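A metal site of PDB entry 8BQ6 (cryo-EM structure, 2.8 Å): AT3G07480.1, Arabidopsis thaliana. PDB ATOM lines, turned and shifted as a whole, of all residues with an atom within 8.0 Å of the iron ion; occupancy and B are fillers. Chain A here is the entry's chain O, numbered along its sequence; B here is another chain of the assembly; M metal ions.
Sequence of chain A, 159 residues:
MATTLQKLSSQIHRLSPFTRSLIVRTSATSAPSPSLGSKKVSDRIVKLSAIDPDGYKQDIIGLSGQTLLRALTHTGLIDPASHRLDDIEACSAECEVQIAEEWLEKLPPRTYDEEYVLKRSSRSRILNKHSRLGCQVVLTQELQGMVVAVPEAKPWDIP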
ATOM      1  N   LEU A  69     -20.855 -20.691 -31.166  1.00  0.00           N
ATOM      2  CA  LEU A  69     -21.530 -20.163 -29.991  1.00  0.00           C
ATOM      3  C   LEU A  69     -22.916 -19.612 -30.340  1.00  0.00           C
ATOM      4  O   LEU A  69     -23.857 -19.776 -29.565  1.00  0.00           O
ATOM      5  CB  LEU A  69     -20.653 -19.094 -29.339  1.00  0.00           C
ATOM      6  CG  LEU A  69     -21.278 -18.257 -28.239  1.00  0.00           C
ATOM      7  CD1 LEU A  69     -21.487 -19.091 -26.990  1.00  0.00           C
ATOM      8  CD2 LEU A  69     -20.390 -17.069 -27.938  1.00  0.00           C
ATOM      9  N   SER A  82     -24.324 -14.881 -21.035  1.00  0.00           N
ATOM     10  CA  SER A  82     -23.002 -15.145 -20.481  1.00  0.00           C
ATOM     11  C   SER A  82     -21.876 -14.853 -21.472  1.00  0.00           C
ATOM     12  O   SER A  82     -20.719 -14.714 -21.054  1.00  0.00           O
ATOM     13  CB  SER A  82     -22.912 -16.594 -20.022  1.00  0.00           C
ATOM     14  OG  SER A  82     -22.642 -17.446 -21.114  1.00  0.00           O
ATOM     15  N   HIS A  83     -22.186 -14.768 -22.764  1.00  0.00           N
ATOM     16  CA  HIS A  83     -21.176 -14.521 -23.789  1.00  0.00           C
ATOM     17  C   HIS A  83     -21.878 -13.722 -24.893  1.00  0.00           C
ATOM     18  O   HIS A  83     -22.325 -14.294 -25.897  1.00  0.00           O
ATOM     19  CB  HIS A  83     -20.618 -15.836 -24.314  1.00  0.00           C
ATOM     20  CG  HIS A  83     -19.232 -15.755 -24.843  1.00  0.00           C
ATOM     21  ND1 HIS A  83     -18.796 -14.751 -25.679  1.00  0.00           N
ATOM     22  CD2 HIS A  83     -18.168 -16.581 -24.682  1.00  0.00           C
ATOM     23  CE1 HIS A  83     -17.537 -14.952 -25.993  1.00  0.00           C
ATOM     24  NE2 HIS A  83     -17.132 -16.057 -25.405  1.00  0.00           N
ATOM     25  N   LEU A  85     -20.571 -11.117 -26.771  1.00  0.00           N
ATOM     26  CA  LEU A  85     -19.705 -10.790 -27.896  1.00  0.00           C
ATOM     27  C   LEU A  85     -19.009 -12.049 -28.407  1.00  0.00           C
ATOM     28  O   LEU A  85     -18.892 -13.054 -27.698  1.00  0.00           O
ATOM     29  CB  LEU A  85     -18.681  -9.720 -27.512  1.00  0.00           C
ATOM     30  CG  LEU A  85     -19.203  -8.454 -26.828  1.00  0.00           C
ATOM     31  CD1 LEU A  85     -18.043  -7.571 -26.385  1.00  0.00           C
ATOM     32  CD2 LEU A  85     -20.118  -7.695 -27.768  1.00  0.00           C
ATOM     33  N   ASP A  86     -18.569 -11.985 -29.658  1.00  0.00           N
ATOM     34  CA  ASP A  86     -17.786 -13.043 -30.289  1.00  0.00           C
ATOM     35  C   ASP A  86     -16.308 -12.691 -30.343  1.00  0.00           C
ATOM     36  O   ASP A  86     -15.627 -12.991 -31.323  1.00  0.00           O
ATOM     37  CB  ASP A  86     -18.303 -13.326 -31.695  1.00  0.00           C
ATOM     38  CG  ASP A  86     -19.574 -14.129 -31.699  1.00  0.00           C
ATOM     39  OD1 ASP A  86     -19.597 -15.224 -31.104  1.00  0.00           O
ATOM     40  OD2 ASP A  86     -20.549 -13.667 -32.326  1.00  0.00           O
ATOM     41  N   ASP A  87     -15.810 -12.026 -29.307  1.00  0.00           N
ATOM     42  CA  ASP A  87     -14.444 -11.550 -29.264  1.00  0.00           C
ATOM     43  C   ASP A  87     -13.675 -12.360 -28.224  1.00  0.00           C
ATOM     44  O   ASP A  87     -14.214 -12.693 -27.167  1.00  0.00           O
ATOM     45  CB  ASP A  87     -14.415 -10.058 -28.905  1.00  0.00           C
ATOM     46  CG  ASP A  87     -13.060  -9.421 -29.153  1.00  0.00           C
ATOM     47  OD1 ASP A  87     -12.951  -8.186 -28.972  1.00  0.00           O
ATOM     48  OD2 ASP A  87     -12.103 -10.131 -29.504  1.00  0.00           O
ATOM     49  N   ILE A  88     -12.421 -12.678 -28.540  1.00  0.00           N
ATOM     50  CA  ILE A  88     -11.590 -13.387 -27.577  1.00  0.00           C
ATOM     51  C   ILE A  88     -11.256 -12.502 -26.384  1.00  0.00           C
ATOM     52  O   ILE A  88     -10.903 -12.985 -25.303  1.00  0.00           O
ATOM     53  CB  ILE A  88     -10.313 -13.925 -28.261  1.00  0.00           C
ATOM     54  CG1 ILE A  88      -9.483 -14.771 -27.295  1.00  0.00           C
ATOM     55  CG2 ILE A  88      -9.481 -12.795 -28.811  1.00  0.00           C
ATOM     56  CD1 ILE A  88      -9.746 -16.226 -27.369  1.00  0.00           C
ATOM     57  N   GLU A  89     -11.393 -11.178 -26.529  1.00  0.00           N
ATOM     58  CA  GLU A  89     -11.129 -10.276 -25.422  1.00  0.00           C
ATOM     59  C   GLU A  89     -12.305 -10.166 -24.466  1.00  0.00           C
ATOM     60  O   GLU A  89     -12.204  -9.479 -23.447  1.00  0.00           O
ATOM     61  CB  GLU A  89     -10.763  -8.890 -25.961  1.00  0.00           C
ATOM     62  CG  GLU A  89      -9.818  -8.934 -27.132  1.00  0.00           C
ATOM     63  CD  GLU A  89      -8.541  -8.156 -26.885  1.00  0.00           C
ATOM     64  OE1 GLU A  89      -8.103  -8.082 -25.709  1.00  0.00           O
ATOM     65  OE2 GLU A  89      -7.971  -7.638 -27.857  1.00  0.00           O
ATOM     66  N   ALA A  90     -13.439 -10.800 -24.772  1.00  0.00           N
ATOM     67  CA  ALA A  90     -14.596 -10.841 -23.894  1.00  0.00           C
ATOM     68  C   ALA A  90     -14.991 -12.282 -23.603  1.00  0.00           C
ATOM     69  O   ALA A  90     -16.171 -12.637 -23.624  1.00  0.00           O
ATOM     70  CB  ALA A  90     -15.760 -10.065 -24.483  1.00  0.00           C
ATOM     71  N   CYS A  91     -14.007 -13.125 -23.347  1.00  0.00           N
ATOM     72  CA  CYS A  91     -14.236 -14.553 -23.204  1.00  0.00           C
ATOM     73  C   CYS A  91     -13.467 -15.084 -22.008  1.00  0.00           C
ATOM     74  O   CYS A  91     -12.254 -14.857 -21.896  1.00  0.00           O
ATOM     75  CB  CYS A  91     -13.820 -15.290 -24.482  1.00  0.00           C
ATOM     76  SG  CYS A  91     -13.585 -17.064 -24.291  1.00  0.00           S
ATOM     77  N   SER A  92     -14.167 -15.778 -21.122  1.00  0.00           N
ATOM     78  CA  SER A  92     -13.556 -16.529 -20.041  1.00  0.00           C
ATOM     79  C   SER A  92     -13.925 -18.007 -20.151  1.00  0.00           C
ATOM     80  O   SER A  92     -14.245 -18.664 -19.160  1.00  0.00           O
ATOM     81  CB  SER A  92     -13.960 -15.979 -18.674  1.00  0.00           C
ATOM     82  OG  SER A  92     -13.555 -14.631 -18.524  1.00  0.00           O
ATOM     83  N   ALA A  93     -13.900 -18.515 -21.380  1.00  0.00           N
ATOM     84  CA  ALA A  93     -14.210 -19.903 -21.699  1.00  0.00           C
ATOM     85  C   ALA A  93     -15.628 -20.298 -21.305  1.00  0.00           C
ATOM     86  O   ALA A  93     -15.916 -21.471 -21.097  1.00  0.00           O
ATOM     87  CB  ALA A  93     -13.201 -20.874 -21.074  1.00  0.00           C
ATOM     88  N   GLU A  94     -16.543 -19.323 -21.207  1.00  0.00           N
ATOM     89  CA  GLU A  94     -17.960 -19.660 -21.059  1.00  0.00           C
ATOM     90  C   GLU A  94     -18.505 -20.334 -22.311  1.00  0.00           C
ATOM     91  O   GLU A  94     -19.575 -20.961 -22.249  1.00  0.00           O
ATOM     92  CB  GLU A  94     -18.777 -18.407 -20.768  1.00  0.00           C
ATOM     93  CG  GLU A  94     -18.380 -17.660 -19.512  1.00  0.00           C
ATOM     94  CD  GLU A  94     -17.399 -16.557 -19.787  1.00  0.00           C
ATOM     95  OE1 GLU A  94     -16.917 -16.448 -20.933  1.00  0.00           O
ATOM     96  OE2 GLU A  94     -17.097 -15.783 -18.854  1.00  0.00           O
ATOM     97  N   CYS A  95     -17.799 -20.220 -23.427  1.00  0.00           N
ATOM     98  CA  CYS A  95     -18.213 -20.815 -24.693  1.00  0.00           C
ATOM     99  C   CYS A  95     -17.528 -22.137 -24.973  1.00  0.00           C
ATOM    100  O   CYS A  95     -17.697 -22.687 -26.063  1.00  0.00           O
ATOM    101  CB  CYS A  95     -17.914 -19.839 -25.829  1.00  0.00           C
ATOM    102  SG  CYS A  95     -16.178 -19.411 -25.940  1.00  0.00           S
ATOM    103  N   GLU A  96     -16.761 -22.662 -24.015  1.00  0.00           N
ATOM    104  CA  GLU A  96     -15.925 -23.818 -24.268  1.00  0.00           C
ATOM    105  C   GLU A  96     -16.764 -25.048 -24.571  1.00  0.00           C
ATOM    106  O   GLU A  96     -17.791 -25.296 -23.934  1.00  0.00           O
ATOM    107  CB  GLU A  96     -15.005 -24.061 -23.067  1.00  0.00           C
ATOM    108  CG  GLU A  96     -14.406 -25.445 -22.995  1.00  0.00           C
ATOM    109  CD  GLU A  96     -13.565 -25.620 -21.744  1.00  0.00           C
ATOM    110  OE1 GLU A  96     -13.679 -24.793 -20.817  1.00  0.00           O
ATOM    111  OE2 GLU A  96     -12.775 -26.590 -21.703  1.00  0.00           O
ATOM    112  N   VAL A 117      -6.555 -18.905 -22.685  1.00  0.00           N
ATOM    113  CA  VAL A 117      -7.852 -18.731 -22.050  1.00  0.00           C
ATOM    114  C   VAL A 117      -8.368 -20.056 -21.513  1.00  0.00           C
ATOM    115  O   VAL A 117      -8.844 -20.155 -20.375  1.00  0.00           O
ATOM    116  CB  VAL A 117      -8.853 -18.088 -23.040  1.00  0.00           C
ATOM    117  CG1 VAL A 117     -10.269 -18.258 -22.547  1.00  0.00           C
ATOM    118  CG2 VAL A 117      -8.534 -16.622 -23.243  1.00  0.00           C
ATOM    119  N   ARG A 132     -12.313 -26.561 -27.365  1.00  0.00           N
ATOM    120  CA  ARG A 132     -12.252 -25.425 -28.262  1.00  0.00           C
ATOM    121  C   ARG A 132     -13.154 -24.324 -27.734  1.00  0.00           C
ATOM    122  O   ARG A 132     -14.211 -24.583 -27.161  1.00  0.00           O
ATOM    123  CB  ARG A 132     -12.704 -25.771 -29.686  1.00  0.00           C
ATOM    124  CG  ARG A 132     -11.950 -26.902 -30.332  1.00  0.00           C
ATOM    125  CD  ARG A 132     -10.605 -26.465 -30.833  1.00  0.00           C
ATOM    126  NE  ARG A 132     -10.630 -25.138 -31.423  1.00  0.00           N
ATOM    127  CZ  ARG A 132     -10.137 -24.862 -32.628  1.00  0.00           C
ATOM    128  NH1 ARG A 132      -9.619 -25.811 -33.393  1.00  0.00           N
ATOM    129  NH2 ARG A 132     -10.178 -23.607 -33.069  1.00  0.00           N
ATOM    130  N   LEU A 133     -12.734 -23.081 -27.953  1.00  0.00           N
ATOM    131  CA  LEU A 133     -13.544 -21.935 -27.589  1.00  0.00           C
ATOM    132  C   LEU A 133     -14.626 -21.746 -28.640  1.00  0.00           C
ATOM    133  O   LEU A 133     -14.334 -21.473 -29.803  1.00  0.00           O
ATOM    134  CB  LEU A 133     -12.670 -20.693 -27.486  1.00  0.00           C
ATOM    135  CG  LEU A 133     -11.851 -20.591 -26.203  1.00  0.00           C
ATOM    136  CD1 LEU A 133     -11.021 -19.339 -26.239  1.00  0.00           C
ATOM    137  CD2 LEU A 133     -12.744 -20.600 -24.996  1.00  0.00           C
ATOM    138  N   GLY A 134     -15.890 -21.900 -28.224  1.00  0.00           N
ATOM    139  CA  GLY A 134     -16.993 -21.817 -29.173  1.00  0.00           C
ATOM    140  C   GLY A 134     -17.101 -20.486 -29.887  1.00  0.00           C
ATOM    141  O   GLY A 134     -17.670 -20.410 -30.974  1.00  0.00           O
ATOM    142  N   CYS A 135     -16.570 -19.423 -29.286  1.00  0.00           N
ATOM    143  CA  CYS A 135     -16.612 -18.111 -29.923  1.00  0.00           C
ATOM    144  C   CYS A 135     -15.604 -17.974 -31.053  1.00  0.00           C
ATOM    145  O   CYS A 135     -15.728 -17.060 -31.872  1.00  0.00           O
ATOM    146  CB  CYS A 135     -16.386 -17.014 -28.891  1.00  0.00           C
ATOM    147  SG  CYS A 135     -14.759 -17.011 -28.122  1.00  0.00           S
ATOM    148  N   GLN A 136     -14.602 -18.857 -31.118  1.00  0.00           N
ATOM    149  CA  GLN A 136     -13.555 -18.787 -32.123  1.00  0.00           C
ATOM    150  C   GLN A 136     -13.732 -19.825 -33.221  1.00  0.00           C
ATOM    151  O   GLN A 136     -12.869 -19.926 -34.106  1.00  0.00           O
ATOM    152  CB  GLN A 136     -12.181 -18.967 -31.484  1.00  0.00           C
ATOM    153  CG  GLN A 136     -11.898 -18.021 -30.345  1.00  0.00           C
ATOM    154  CD  GLN A 136     -11.679 -16.609 -30.812  1.00  0.00           C
ATOM    155  OE1 GLN A 136     -10.645 -16.299 -31.415  1.00  0.00           O
ATOM    156  NE2 GLN A 136     -12.643 -15.732 -30.545  1.00  0.00           N
ATOM    157  N   TYR B 373     -16.297  -6.792 -19.249  1.00  0.00           N
ATOM    158  CA  TYR B 373     -15.035  -6.699 -19.964  1.00  0.00           C
ATOM    159  C   TYR B 373     -14.813  -5.303 -20.502  1.00  0.00           C
ATOM    160  O   TYR B 373     -15.747  -4.527 -20.689  1.00  0.00           O
ATOM    161  CB  TYR B 373     -15.008  -7.697 -21.132  1.00  0.00           C
ATOM    162  CG  TYR B 373     -15.133  -9.144 -20.724  1.00  0.00           C
ATOM    163  CD1 TYR B 373     -14.046  -9.851 -20.262  1.00  0.00           C
ATOM    164  CD2 TYR B 373     -16.347  -9.796 -20.810  1.00  0.00           C
ATOM    165  CE1 TYR B 373     -14.152 -11.176 -19.888  1.00  0.00           C
ATOM    166  CE2 TYR B 373     -16.475 -11.117 -20.448  1.00  0.00           C
ATOM    167  CZ  TYR B 373     -15.378 -11.802 -19.988  1.00  0.00           C
ATOM    168  OH  TYR B 373     -15.506 -13.124 -19.626  1.00  0.00           O
HETATM  169 FE    FE M   1     -15.409 -17.361 -25.531  1.00  0.00          FE
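The side-chain sulfur (SG) of Cys 135 sits close to the side-chain amide nitrogen (NE2) of Gln 136, 3.5 Å away. ND1 of His 83 is in hydrogen-bond range of O of Leu 85, 2.6 Å away. The backbone carbonyl oxygen (O) of Cys 95 lies within hydrogen-bond range of the backbone NH (N) of Gly 134 (2.9 Å). The side-chain sulfur (SG) of Cys 91 sits close to the backbone NH (N) of Ala 93 (3.3 Å).
Of the 22 residues printed, 4 come within 4 Å of the iron ion. The nearest printed residue that does not touch the iron ion is Leu 133 (4.2 Å).
The iron ion is bound by a ring nitrogen (NE2) of His 83, the side-chain sulfur (SG) of Cys 91, the side-chain sulfur (SG) of Cys 95 and the side-chain sulfur (SG) of Cys 135.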
